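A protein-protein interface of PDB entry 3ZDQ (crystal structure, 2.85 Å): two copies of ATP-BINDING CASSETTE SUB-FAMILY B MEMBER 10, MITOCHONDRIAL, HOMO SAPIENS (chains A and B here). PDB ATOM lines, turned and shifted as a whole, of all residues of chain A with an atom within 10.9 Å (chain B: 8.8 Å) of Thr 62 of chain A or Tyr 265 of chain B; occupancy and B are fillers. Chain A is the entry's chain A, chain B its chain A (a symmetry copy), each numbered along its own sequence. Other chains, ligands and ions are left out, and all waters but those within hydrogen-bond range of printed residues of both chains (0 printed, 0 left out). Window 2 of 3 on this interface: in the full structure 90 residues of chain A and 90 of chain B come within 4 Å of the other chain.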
ATOM      1  N   LEU A  42     -30.498  -8.085 -10.603  1.00  0.00           N
ATOM      2  CA  LEU A  42     -29.055  -7.888 -10.523  1.00  0.00           C
ATOM      3  C   LEU A  42     -28.578  -6.983 -11.685  1.00  0.00           C
ATOM      4  O   LEU A  42     -27.774  -6.088 -11.445  1.00  0.00           O
ATOM      5  CB  LEU A  42     -28.320  -9.232 -10.512  1.00  0.00           C
ATOM      6  CG  LEU A  42     -26.923  -9.232  -9.920  1.00  0.00           C
ATOM      7  CD1 LEU A  42     -26.959  -9.028  -8.412  1.00  0.00           C
ATOM      8  CD2 LEU A  42     -26.219 -10.538 -10.243  1.00  0.00           C
ATOM      9  N   ILE A  45     -29.322  -3.381 -10.827  1.00  0.00           N
ATOM     10  CA  ILE A  45     -28.364  -2.883  -9.826  1.00  0.00           C
ATOM     11  C   ILE A  45     -27.010  -2.591 -10.520  1.00  0.00           C
ATOM     12  O   ILE A  45     -26.432  -1.527 -10.267  1.00  0.00           O
ATOM     13  CB  ILE A  45     -28.241  -3.859  -8.604  1.00  0.00           C
ATOM     14  CG1 ILE A  45     -29.508  -3.759  -7.700  1.00  0.00           C
ATOM     15  CG2 ILE A  45     -26.930  -3.642  -7.787  1.00  0.00           C
ATOM     16  CD1 ILE A  45     -29.856  -4.983  -6.945  1.00  0.00           C
ATOM     17  N   ILE A  49     -25.143   1.081 -10.454  1.00  0.00           N
ATOM     18  CA  ILE A  49     -23.770   1.368 -10.039  1.00  0.00           C
ATOM     19  C   ILE A  49     -23.023   2.057 -11.189  1.00  0.00           C
ATOM     20  O   ILE A  49     -22.415   3.106 -10.965  1.00  0.00           O
ATOM     21  CB  ILE A  49     -23.014   0.114  -9.562  1.00  0.00           C
ATOM     22  CG1 ILE A  49     -23.775  -0.640  -8.457  1.00  0.00           C
ATOM     23  CG2 ILE A  49     -21.604   0.496  -9.089  1.00  0.00           C
ATOM     24  CD1 ILE A  49     -23.472  -2.185  -8.475  1.00  0.00           C
ATOM     25  N   ASP A  56     -23.469   7.685  -2.932  1.00  0.00           N
ATOM     26  CA  ASP A  56     -23.336   6.831  -1.757  1.00  0.00           C
ATOM     27  C   ASP A  56     -24.504   5.872  -1.768  1.00  0.00           C
ATOM     28  O   ASP A  56     -25.648   6.335  -1.779  1.00  0.00           O
ATOM     29  CB  ASP A  56     -23.318   7.672  -0.478  1.00  0.00           C
ATOM     30  CG  ASP A  56     -22.836   6.975   0.782  1.00  0.00           C
ATOM     31  OD1 ASP A  56     -23.224   5.817   1.008  1.00  0.00           O
ATOM     32  OD2 ASP A  56     -22.157   7.631   1.595  1.00  0.00           O
ATOM     33  N   TYR A  57     -24.225   4.542  -1.804  1.00  0.00           N
ATOM     34  CA  TYR A  57     -25.251   3.496  -1.850  1.00  0.00           C
ATOM     35  C   TYR A  57     -25.292   2.613  -0.592  1.00  0.00           C
ATOM     36  O   TYR A  57     -26.003   1.601  -0.592  1.00  0.00           O
ATOM     37  CB  TYR A  57     -25.056   2.621  -3.098  1.00  0.00           C
ATOM     38  CG  TYR A  57     -25.484   3.299  -4.381  1.00  0.00           C
ATOM     39  CD1 TYR A  57     -26.825   3.587  -4.626  1.00  0.00           C
ATOM     40  CD2 TYR A  57     -24.553   3.626  -5.367  1.00  0.00           C
ATOM     41  CE1 TYR A  57     -27.221   4.236  -5.791  1.00  0.00           C
ATOM     42  CE2 TYR A  57     -24.944   4.240  -6.557  1.00  0.00           C
ATOM     43  CZ  TYR A  57     -26.282   4.539  -6.762  1.00  0.00           C
ATOM     44  OH  TYR A  57     -26.696   5.139  -7.920  1.00  0.00           O
ATOM     45  N   SER A  58     -24.604   3.035   0.495  1.00  0.00           N
ATOM     46  CA  SER A  58     -24.515   2.311   1.774  1.00  0.00           C
ATOM     47  C   SER A  58     -25.873   1.969   2.379  1.00  0.00           C
ATOM     48  O   SER A  58     -26.046   0.839   2.832  1.00  0.00           O
ATOM     49  CB  SER A  58     -23.725   3.116   2.800  1.00  0.00           C
ATOM     50  OG  SER A  58     -22.406   3.400   2.370  1.00  0.00           O
ATOM     51  N   ASP A  59     -26.819   2.936   2.413  1.00  0.00           N
ATOM     52  CA  ASP A  59     -28.132   2.722   3.014  1.00  0.00           C
ATOM     53  C   ASP A  59     -28.984   1.793   2.197  1.00  0.00           C
ATOM     54  O   ASP A  59     -29.651   0.941   2.774  1.00  0.00           O
ATOM     55  CB  ASP A  59     -28.871   4.037   3.273  1.00  0.00           C
ATOM     56  CG  ASP A  59     -28.909   4.435   4.737  1.00  0.00           C
ATOM     57  OD1 ASP A  59     -28.117   3.866   5.535  1.00  0.00           O
ATOM     58  OD2 ASP A  59     -29.753   5.290   5.097  1.00  0.00           O
ATOM     59  N   ASN A  60     -28.936   1.909   0.877  1.00  0.00           N
ATOM     60  CA  ASN A  60     -29.660   1.006  -0.026  1.00  0.00           C
ATOM     61  C   ASN A  60     -29.151  -0.416   0.116  1.00  0.00           C
ATOM     62  O   ASN A  60     -29.949  -1.342   0.188  1.00  0.00           O
ATOM     63  CB  ASN A  60     -29.516   1.459  -1.481  1.00  0.00           C
ATOM     64  CG  ASN A  60     -29.972   2.870  -1.671  1.00  0.00           C
ATOM     65  OD1 ASN A  60     -29.162   3.811  -1.659  1.00  0.00           O
ATOM     66  ND2 ASN A  60     -31.287   3.039  -1.737  1.00  0.00           N
ATOM     67  N   LEU A  61     -27.818  -0.568   0.181  1.00  0.00           N
ATOM     68  CA  LEU A  61     -27.121  -1.833   0.328  1.00  0.00           C
ATOM     69  C   LEU A  61     -27.479  -2.481   1.678  1.00  0.00           C
ATOM     70  O   LEU A  61     -27.876  -3.645   1.688  1.00  0.00           O
ATOM     71  CB  LEU A  61     -25.611  -1.590   0.187  1.00  0.00           C
ATOM     72  CG  LEU A  61     -24.655  -2.783   0.241  1.00  0.00           C
ATOM     73  CD1 LEU A  61     -24.948  -3.799  -0.848  1.00  0.00           C
ATOM     74  CD2 LEU A  61     -23.235  -2.300   0.121  1.00  0.00           C
ATOM     75  N   THR A  62     -27.423  -1.718   2.787  1.00  0.00           N
ATOM     76  CA  THR A  62     -27.781  -2.218   4.111  1.00  0.00           C
ATOM     77  C   THR A  62     -29.261  -2.647   4.137  1.00  0.00           C
ATOM     78  O   THR A  62     -29.555  -3.713   4.676  1.00  0.00           O
ATOM     79  CB  THR A  62     -27.470  -1.174   5.189  1.00  0.00           C
ATOM     80  OG1 THR A  62     -26.153  -0.671   4.989  1.00  0.00           O
ATOM     81  CG2 THR A  62     -27.560  -1.741   6.583  1.00  0.00           C
ATOM     82  N   ARG A  63     -30.177  -1.851   3.536  1.00  0.00           N
ATOM     83  CA  ARG A  63     -31.602  -2.212   3.478  1.00  0.00           C
ATOM     84  C   ARG A  63     -31.825  -3.453   2.614  1.00  0.00           C
ATOM     85  O   ARG A  63     -32.570  -4.356   3.013  1.00  0.00           O
ATOM     86  CB  ARG A  63     -32.457  -1.055   2.958  1.00  0.00           C
ATOM     87  CG  ARG A  63     -32.875  -0.106   4.054  1.00  0.00           C
ATOM     88  CD  ARG A  63     -33.228   1.299   3.586  1.00  0.00           C
ATOM     89  NE  ARG A  63     -33.612   2.146   4.726  1.00  0.00           N
ATOM     90  CZ  ARG A  63     -32.756   2.797   5.515  1.00  0.00           C
ATOM     91  NH1 ARG A  63     -31.448   2.732   5.288  1.00  0.00           N
ATOM     92  NH2 ARG A  63     -33.202   3.516   6.538  1.00  0.00           N
ATOM     93  N   LEU A  64     -31.144  -3.519   1.452  1.00  0.00           N
ATOM     94  CA  LEU A  64     -31.237  -4.638   0.516  1.00  0.00           C
ATOM     95  C   LEU A  64     -30.719  -5.936   1.137  1.00  0.00           C
ATOM     96  O   LEU A  64     -31.357  -6.977   0.979  1.00  0.00           O
ATOM     97  CB  LEU A  64     -30.491  -4.339  -0.783  1.00  0.00           C
ATOM     98  CG  LEU A  64     -30.791  -5.310  -1.903  1.00  0.00           C
ATOM     99  CD1 LEU A  64     -32.196  -5.093  -2.475  1.00  0.00           C
ATOM    100  CD2 LEU A  64     -29.720  -5.241  -2.983  1.00  0.00           C
ATOM    101  N   CYS A  65     -29.581  -5.866   1.851  1.00  0.00           N
ATOM    102  CA  CYS A  65     -28.970  -7.018   2.505  1.00  0.00           C
ATOM    103  C   CYS A  65     -29.785  -7.456   3.721  1.00  0.00           C
ATOM    104  O   CYS A  65     -29.838  -8.655   3.990  1.00  0.00           O
ATOM    105  CB  CYS A  65     -27.516  -6.735   2.862  1.00  0.00           C
ATOM    106  SG  CYS A  65     -26.450  -6.516   1.410  1.00  0.00           S
ATOM    107  N   LEU A  66     -30.470  -6.522   4.411  1.00  0.00           N
ATOM    108  CA  LEU A  66     -31.360  -6.892   5.510  1.00  0.00           C
ATOM    109  C   LEU A  66     -32.626  -7.549   4.931  1.00  0.00           C
ATOM    110  O   LEU A  66     -33.058  -8.589   5.438  1.00  0.00           O
ATOM    111  CB  LEU A  66     -31.705  -5.701   6.407  1.00  0.00           C
ATOM    112  CG  LEU A  66     -30.663  -5.353   7.466  1.00  0.00           C
ATOM    113  CD1 LEU A  66     -30.950  -4.001   8.085  1.00  0.00           C
ATOM    114  CD2 LEU A  66     -30.580  -6.416   8.546  1.00  0.00           C
ATOM    115  N   GLY A  67     -33.141  -6.980   3.830  1.00  0.00           N
ATOM    116  CA  GLY A  67     -34.286  -7.504   3.088  1.00  0.00           C
ATOM    117  C   GLY A  67     -33.994  -8.869   2.486  1.00  0.00           C
ATOM    118  O   GLY A  67     -34.812  -9.786   2.618  1.00  0.00           O
ATOM    119  N   LEU A  68     -32.794  -9.046   1.872  1.00  0.00           N
ATOM    120  CA  LEU A  68     -32.389 -10.335   1.299  1.00  0.00           C
ATOM    121  C   LEU A  68     -32.198 -11.407   2.381  1.00  0.00           C
ATOM    122  O   LEU A  68     -32.481 -12.571   2.102  1.00  0.00           O
ATOM    123  CB  LEU A  68     -31.130 -10.232   0.442  1.00  0.00           C
ATOM    124  CG  LEU A  68     -31.290  -9.679  -0.975  1.00  0.00           C
ATOM    125  CD1 LEU A  68     -29.965  -9.647  -1.666  1.00  0.00           C
ATOM    126  CD2 LEU A  68     -32.269 -10.496  -1.816  1.00  0.00           C
ATOM    127  N   SER A  69     -31.765 -11.026   3.612  1.00  0.00           N
ATOM    128  CA  SER A  69     -31.628 -11.952   4.748  1.00  0.00           C
ATOM    129  C   SER A  69     -32.973 -12.601   5.042  1.00  0.00           C
ATOM    130  O   SER A  69     -33.044 -13.821   5.186  1.00  0.00           O
ATOM    131  CB  SER A  69     -31.141 -11.221   5.998  1.00  0.00           C
ATOM    132  OG  SER A  69     -29.805 -10.772   5.883  1.00  0.00           O
ATOM    133  N   ALA A  70     -34.046 -11.755   5.106  1.00  0.00           N
ATOM    134  CA  ALA A  70     -35.433 -12.153   5.346  1.00  0.00           C
ATOM    135  C   ALA A  70     -35.921 -13.067   4.234  1.00  0.00           C
ATOM    136  O   ALA A  70     -36.513 -14.107   4.546  1.00  0.00           O
ATOM    137  CB  ALA A  70     -36.326 -10.929   5.449  1.00  0.00           C
ATOM    138  N   PHE A  72     -33.991 -14.946   2.218  1.00  0.00           N
ATOM    139  CA  PHE A  72     -33.211 -16.172   2.395  1.00  0.00           C
ATOM    140  C   PHE A  72     -33.729 -17.044   3.542  1.00  0.00           C
ATOM    141  O   PHE A  72     -33.729 -18.263   3.388  1.00  0.00           O
ATOM    142  CB  PHE A  72     -31.722 -15.863   2.601  1.00  0.00           C
ATOM    143  CG  PHE A  72     -31.025 -15.390   1.348  1.00  0.00           C
ATOM    144  CD1 PHE A  72     -31.280 -15.988   0.123  1.00  0.00           C
ATOM    145  CD2 PHE A  72     -30.082 -14.379   1.400  1.00  0.00           C
ATOM    146  CE1 PHE A  72     -30.648 -15.543  -1.032  1.00  0.00           C
ATOM    147  CE2 PHE A  72     -29.462 -13.918   0.233  1.00  0.00           C
ATOM    148  CZ  PHE A  72     -29.743 -14.512  -0.973  1.00  0.00           C
ATOM    149  N   LEU B 164     -11.244  -8.711   2.989  1.00  0.00           N
ATOM    150  CA  LEU B 164     -12.323  -9.638   2.641  1.00  0.00           C
ATOM    151  C   LEU B 164     -11.876 -11.103   2.768  1.00  0.00           C
ATOM    152  O   LEU B 164     -12.665 -11.914   3.268  1.00  0.00           O
ATOM    153  CB  LEU B 164     -12.867  -9.379   1.241  1.00  0.00           C
ATOM    154  CG  LEU B 164     -13.886  -8.287   1.058  1.00  0.00           C
ATOM    155  CD1 LEU B 164     -14.185  -8.121  -0.399  1.00  0.00           C
ATOM    156  CD2 LEU B 164     -15.181  -8.642   1.736  1.00  0.00           C
ATOM    157  N   PHE B 167     -11.802 -11.968   6.459  1.00  0.00           N
ATOM    158  CA  PHE B 167     -13.198 -12.049   6.880  1.00  0.00           C
ATOM    159  C   PHE B 167     -13.756 -13.460   6.531  1.00  0.00           C
ATOM    160  O   PHE B 167     -14.150 -14.191   7.440  1.00  0.00           O
ATOM    161  CB  PHE B 167     -14.008 -10.905   6.207  1.00  0.00           C
ATOM    162  CG  PHE B 167     -15.507 -11.017   6.332  1.00  0.00           C
ATOM    163  CD1 PHE B 167     -16.143 -10.709   7.527  1.00  0.00           C
ATOM    164  CD2 PHE B 167     -16.281 -11.456   5.261  1.00  0.00           C
ATOM    165  CE1 PHE B 167     -17.518 -10.872   7.667  1.00  0.00           C
ATOM    166  CE2 PHE B 167     -17.666 -11.598   5.391  1.00  0.00           C
ATOM    167  CZ  PHE B 167     -18.274 -11.311   6.598  1.00  0.00           C
ATOM    168  N   LEU B 258     -26.213 -16.536   3.326  1.00  0.00           N
ATOM    169  CA  LEU B 258     -25.831 -15.445   4.236  1.00  0.00           C
ATOM    170  C   LEU B 258     -24.320 -15.155   4.192  1.00  0.00           C
ATOM    171  O   LEU B 258     -23.938 -13.993   4.292  1.00  0.00           O
ATOM    172  CB  LEU B 258     -26.251 -15.723   5.688  1.00  0.00           C
ATOM    173  CG  LEU B 258     -27.757 -15.758   6.014  1.00  0.00           C
ATOM    174  CD1 LEU B 258     -27.977 -16.157   7.463  1.00  0.00           C
ATOM    175  CD2 LEU B 258     -28.448 -14.423   5.718  1.00  0.00           C
ATOM    176  N   ILE B 259     -23.470 -16.183   4.015  1.00  0.00           N
ATOM    177  CA  ILE B 259     -22.012 -15.996   3.923  1.00  0.00           C
ATOM    178  C   ILE B 259     -21.696 -15.181   2.666  1.00  0.00           C
ATOM    179  O   ILE B 259     -21.007 -14.161   2.781  1.00  0.00           O
ATOM    180  CB  ILE B 259     -21.219 -17.340   3.999  1.00  0.00           C
ATOM    181  CG1 ILE B 259     -21.149 -17.820   5.473  1.00  0.00           C
ATOM    182  CG2 ILE B 259     -19.802 -17.197   3.393  1.00  0.00           C
ATOM    183  CD1 ILE B 259     -20.818 -19.222   5.694  1.00  0.00           C
ATOM    184  N   VAL B 260     -22.242 -15.588   1.492  1.00  0.00           N
ATOM    185  CA  VAL B 260     -22.088 -14.866   0.211  1.00  0.00           C
ATOM    186  C   VAL B 260     -22.603 -13.417   0.359  1.00  0.00           C
ATOM    187  O   VAL B 260     -21.908 -12.487  -0.055  1.00  0.00           O
ATOM    188  CB  VAL B 260     -22.819 -15.605  -0.934  1.00  0.00           C
ATOM    189  CG1 VAL B 260     -22.732 -14.842  -2.244  1.00  0.00           C
ATOM    190  CG2 VAL B 260     -22.292 -17.018  -1.089  1.00  0.00           C
ATOM    191  N   LEU B 261     -23.799 -13.235   0.989  1.00  0.00           N
ATOM    192  CA  LEU B 261     -24.443 -11.941   1.223  1.00  0.00           C
ATOM    193  C   LEU B 261     -23.541 -11.033   2.046  1.00  0.00           C
ATOM    194  O   LEU B 261     -23.435  -9.854   1.731  1.00  0.00           O
ATOM    195  CB  LEU B 261     -25.803 -12.135   1.920  1.00  0.00           C
ATOM    196  CG  LEU B 261     -26.710 -10.911   1.994  1.00  0.00           C
ATOM    197  CD1 LEU B 261     -27.066 -10.410   0.610  1.00  0.00           C
ATOM    198  CD2 LEU B 261     -27.961 -11.212   2.796  1.00  0.00           C
ATOM    199  N   SER B 262     -22.868 -11.591   3.072  1.00  0.00           N
ATOM    200  CA  SER B 262     -21.918 -10.878   3.928  1.00  0.00           C
ATOM    201  C   SER B 262     -20.720 -10.333   3.120  1.00  0.00           C
ATOM    202  O   SER B 262     -20.231  -9.233   3.400  1.00  0.00           O
ATOM    203  CB  SER B 262     -21.402 -11.815   5.013  1.00  0.00           C
ATOM    204  OG  SER B 262     -22.468 -12.265   5.826  1.00  0.00           O
ATOM    205  N   VAL B 263     -20.244 -11.124   2.141  1.00  0.00           N
ATOM    206  CA  VAL B 263     -19.123 -10.772   1.288  1.00  0.00           C
ATOM    207  C   VAL B 263     -19.575  -9.661   0.336  1.00  0.00           C
ATOM    208  O   VAL B 263     -18.839  -8.681   0.178  1.00  0.00           O
ATOM    209  CB  VAL B 263     -18.535 -12.009   0.557  1.00  0.00           C
ATOM    210  CG1 VAL B 263     -17.355 -11.630  -0.340  1.00  0.00           C
ATOM    211  CG2 VAL B 263     -18.118 -13.091   1.551  1.00  0.00           C
ATOM    212  N   LEU B 264     -20.804  -9.757  -0.218  1.00  0.00           N
ATOM    213  CA  LEU B 264     -21.336  -8.723  -1.111  1.00  0.00           C
ATOM    214  C   LEU B 264     -21.546  -7.397  -0.372  1.00  0.00           C
ATOM    215  O   LEU B 264     -21.270  -6.331  -0.922  1.00  0.00           O
ATOM    216  CB  LEU B 264     -22.641  -9.181  -1.758  1.00  0.00           C
ATOM    217  CG  LEU B 264     -22.502 -10.278  -2.795  1.00  0.00           C
ATOM    218  CD1 LEU B 264     -23.808 -10.997  -2.995  1.00  0.00           C
ATOM    219  CD2 LEU B 264     -21.991  -9.728  -4.093  1.00  0.00           C
ATOM    220  N   TYR B 265     -21.996  -7.473   0.889  1.00  0.00           N
ATOM    221  CA  TYR B 265     -22.222  -6.335   1.768  1.00  0.00           C
ATOM    222  C   TYR B 265     -20.897  -5.704   2.207  1.00  0.00           C
ATOM    223  O   TYR B 265     -20.715  -4.512   2.015  1.00  0.00           O
ATOM    224  CB  TYR B 265     -23.050  -6.766   2.979  1.00  0.00           C
ATOM    225  CG  TYR B 265     -23.339  -5.633   3.932  1.00  0.00           C
ATOM    226  CD1 TYR B 265     -24.103  -4.538   3.532  1.00  0.00           C
ATOM    227  CD2 TYR B 265     -22.823  -5.634   5.223  1.00  0.00           C
ATOM    228  CE1 TYR B 265     -24.338  -3.470   4.395  1.00  0.00           C
ATOM    229  CE2 TYR B 265     -23.065  -4.576   6.099  1.00  0.00           C
ATOM    230  CZ  TYR B 265     -23.812  -3.491   5.675  1.00  0.00           C
ATOM    231  OH  TYR B 265     -24.028  -2.432   6.515  1.00  0.00           O
ATOM    232  N   LYS B 266     -19.965  -6.482   2.776  1.00  0.00           N
ATOM    233  CA  LYS B 266     -18.660  -5.947   3.205  1.00  0.00           C
ATOM    234  C   LYS B 266     -17.909  -5.364   2.004  1.00  0.00           C
ATOM    235  O   LYS B 266     -17.337  -4.270   2.129  1.00  0.00           O
ATOM    236  CB  LYS B 266     -17.814  -7.020   3.915  1.00  0.00           C
ATOM    237  CG  LYS B 266     -16.604  -6.474   4.675  1.00  0.00           C
ATOM    238  CD  LYS B 266     -16.548  -7.099   6.051  1.00  0.00           C
ATOM    239  CE  LYS B 266     -15.176  -7.162   6.643  1.00  0.00           C
ATOM    240  NZ  LYS B 266     -14.619  -5.824   6.905  1.00  0.00           N
ATOM    241  N   GLY B 267     -17.948  -6.089   0.867  1.00  0.00           N
ATOM    242  CA  GLY B 267     -17.357  -5.678  -0.406  1.00  0.00           C
ATOM    243  C   GLY B 267     -17.988  -4.405  -0.947  1.00  0.00           C
ATOM    244  O   GLY B 267     -17.279  -3.488  -1.398  1.00  0.00           O
ATOM    245  N   GLY B 268     -19.322  -4.327  -0.854  1.00  0.00           N
ATOM    246  CA  GLY B 268     -20.088  -3.162  -1.267  1.00  0.00           C
ATOM    247  C   GLY B 268     -19.676  -1.914  -0.505  1.00  0.00           C
ATOM    248  O   GLY B 268     -19.520  -0.839  -1.101  1.00  0.00           O
ATOM    249  N   LEU B 269     -19.453  -2.066   0.827  1.00  0.00           N
ATOM    250  CA  LEU B 269     -19.018  -0.981   1.699  1.00  0.00           C
ATOM    251  C   LEU B 269     -17.585  -0.575   1.389  1.00  0.00           C
ATOM    252  O   LEU B 269     -17.289   0.621   1.417  1.00  0.00           O
ATOM    253  CB  LEU B 269     -19.143  -1.337   3.191  1.00  0.00           C
ATOM    254  CG  LEU B 269     -20.529  -1.700   3.744  1.00  0.00           C
ATOM    255  CD1 LEU B 269     -20.393  -2.379   5.103  1.00  0.00           C
ATOM    256  CD2 LEU B 269     -21.473  -0.491   3.811  1.00  0.00           C
ATOM    257  N   LEU B 270     -16.696  -1.559   1.076  1.00  0.00           N
ATOM    258  CA  LEU B 270     -15.286  -1.313   0.747  1.00  0.00           C
ATOM    259  C   LEU B 270     -15.151  -0.554  -0.580  1.00  0.00           C
ATOM    260  O   LEU B 270     -14.243   0.256  -0.713  1.00  0.00           O
ATOM    261  CB  LEU B 270     -14.463  -2.599   0.746  1.00  0.00           C
ATOM    262  CG  LEU B 270     -14.112  -3.180   2.127  1.00  0.00           C
ATOM    263  CD1 LEU B 270     -13.580  -4.568   2.013  1.00  0.00           C
ATOM    264  CD2 LEU B 270     -13.108  -2.309   2.876  1.00  0.00           C
ATOM    265  N   MET B 271     -16.091  -0.757  -1.517  1.00  0.00           N
ATOM    266  CA  MET B 271     -16.176  -0.027  -2.782  1.00  0.00           C
ATOM    267  C   MET B 271     -16.532   1.442  -2.524  1.00  0.00           C
ATOM    268  O   MET B 271     -15.873   2.347  -3.044  1.00  0.00           O
ATOM    269  CB  MET B 271     -17.244  -0.642  -3.685  1.00  0.00           C
ATOM    270  CG  MET B 271     -16.834  -1.901  -4.368  1.00  0.00           C
ATOM    271  SD  MET B 271     -17.966  -2.144  -5.752  1.00  0.00           S
ATOM    272  CE  MET B 271     -18.937  -3.317  -5.117  1.00  0.00           C
ATOM    273  N   GLY B 272     -17.577   1.659  -1.716  1.00  0.00           N
ATOM    274  CA  GLY B 272     -18.062   2.985  -1.329  1.00  0.00           C
ATOM    275  C   GLY B 272     -17.004   3.845  -0.668  1.00  0.00           C
ATOM    276  O   GLY B 272     -16.918   5.039  -0.959  1.00  0.00           O
ATOM    277  N   MET B 276     -11.866  -0.616  -2.805  1.00  0.00           N
ATOM    278  CA  MET B 276     -12.023  -1.590  -3.883  1.00  0.00           C
ATOM    279  C   MET B 276     -12.818  -1.067  -5.061  1.00  0.00           C
ATOM    280  O   MET B 276     -13.650  -0.168  -4.886  1.00  0.00           O
ATOM    281  CB  MET B 276     -12.803  -2.776  -3.333  1.00  0.00           C
ATOM    282  CG  MET B 276     -11.979  -3.894  -2.875  1.00  0.00           C
ATOM    283  SD  MET B 276     -13.015  -5.370  -2.894  1.00  0.00           S
ATOM    284  CE  MET B 276     -14.339  -4.794  -2.023  1.00  0.00           C
ATOM    285  N   LEU B 281     -13.969  -6.562  -6.836  1.00  0.00           N
ATOM    286  CA  LEU B 281     -14.934  -7.382  -6.106  1.00  0.00           C
ATOM    287  C   LEU B 281     -15.341  -8.582  -6.957  1.00  0.00           C
ATOM    288  O   LEU B 281     -15.261  -9.704  -6.452  1.00  0.00           O
ATOM    289  CB  LEU B 281     -16.162  -6.611  -5.632  1.00  0.00           C
ATOM    290  CG  LEU B 281     -17.118  -7.413  -4.717  1.00  0.00           C
ATOM    291  CD1 LEU B 281     -16.433  -7.881  -3.420  1.00  0.00           C
ATOM    292  CD2 LEU B 281     -18.372  -6.631  -4.398  1.00  0.00           C
ATOM    293  N   LEU B 285     -15.031 -12.536  -5.851  1.00  0.00           N
ATOM    294  CA  LEU B 285     -16.130 -13.493  -5.790  1.00  0.00           C
ATOM    295  C   LEU B 285     -15.871 -14.707  -6.680  1.00  0.00           C
ATOM    296  O   LEU B 285     -16.095 -15.824  -6.228  1.00  0.00           O
ATOM    297  CB  LEU B 285     -17.469 -12.832  -6.129  1.00  0.00           C
ATOM    298  CG  LEU B 285     -17.963 -11.834  -5.074  1.00  0.00           C
ATOM    299  CD1 LEU B 285     -18.913 -10.799  -5.696  1.00  0.00           C
ATOM    300  CD2 LEU B 285     -18.508 -12.538  -3.803  1.00  0.00           C
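Asp 56 of chain A touches none of the printed residues of chain B.
Of chain B, only Tyr 265 (3.8 Å), Gly 268 (3.5 Å) and Leu 269 (3.9 Å) come within 4 Å of Leu 61 of chain A.
Of chain B, only Tyr 265 comes within 4 Å of Thr 62 of chain A.
Of the printed residues of chain B, Leu 68 of chain A touches Leu 261.
Of the printed residues of chain A, Leu 258 of chain B touches Ser 69.
No residue of chain A comes within 4 Å of Ser 262 of chain B.
No residue of chain A comes within 4 Å of Leu 264 of chain B.
Of chain A, only Leu 61 (3.8 Å), Thr 62 (3.2 Å) and Cys 65 (3.7 Å) come within 4 Å of Tyr 265 of chain B.
Of chain A, only Leu 61 comes within 4 Å of Gly 268 of chain B.
The nearest printed residue of chain A that does not touch Leu 258 of chain B is Phe 72 of chain A (4.6 Å).
Tyr 265 of chain B touches Leu 61 of chain A.
Gly 268 of chain B touches Leu 61 of chain A.
N of Leu 269 of chain B touches CD2 of Leu 61 of chain A, at 3.9 Å.
Cys 65 of chain A touches Leu 261 of chain B.
CD1 of Tyr 265 of chain B touches SG of Cys 65 of chain A, 3.7 Å away.
Leu 68 of chain A touches Leu 261 of chain B (CD1 to CD1, 3.8 Å).
Leu 258 of chain B touches Ser 69 of chain A.
Leu 261 of chain B touches Ser 69 of chain A.
The side-chain hydroxyl of Thr 62 of chain A is in hydrogen-bond range of the side-chain hydroxyl of Tyr 265 of chain B, 3.2 Å away.
Of the 19 printed residues of chain A, 5 touch a printed residue of chain B.
Of the 20 printed residues of chain B, 5 touch a printed residue of chain A.
Printed residues of chain B that touch a printed residue of chain A: Leu 258, Leu 261, Tyr 265, Gly 268 and Leu 269.
Hydrophobic or aromatic side chains of chain B within 4 Å of the printed part of chain A: Leu 258, Leu 261 and Tyr 265.
Among the printed residues, 9 pairs touch across the chains.
No position is printed for both chains.
Of the 9 pairs that touch across the chains among the printed residues, none has its exchanged pair printed and touching as well.
The backbone carbonyl oxygen of Ser 58 of chain A sits at hydrogen-bond distance from the side-chain hydroxyl of Thr 62 of chain A, at 2.6 Å.
O of Leu 61 of chain A sits at hydrogen-bond distance from SG of Cys 65 of chain A (3.2 Å).
OG of Ser 69 of chain A sits at hydrogen-bond distance from O of Cys 65 of chain A (2.8 Å).
O of Leu 258 of chain B sits at hydrogen-bond distance from OG of Ser 262 of chain B (2.7 Å).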
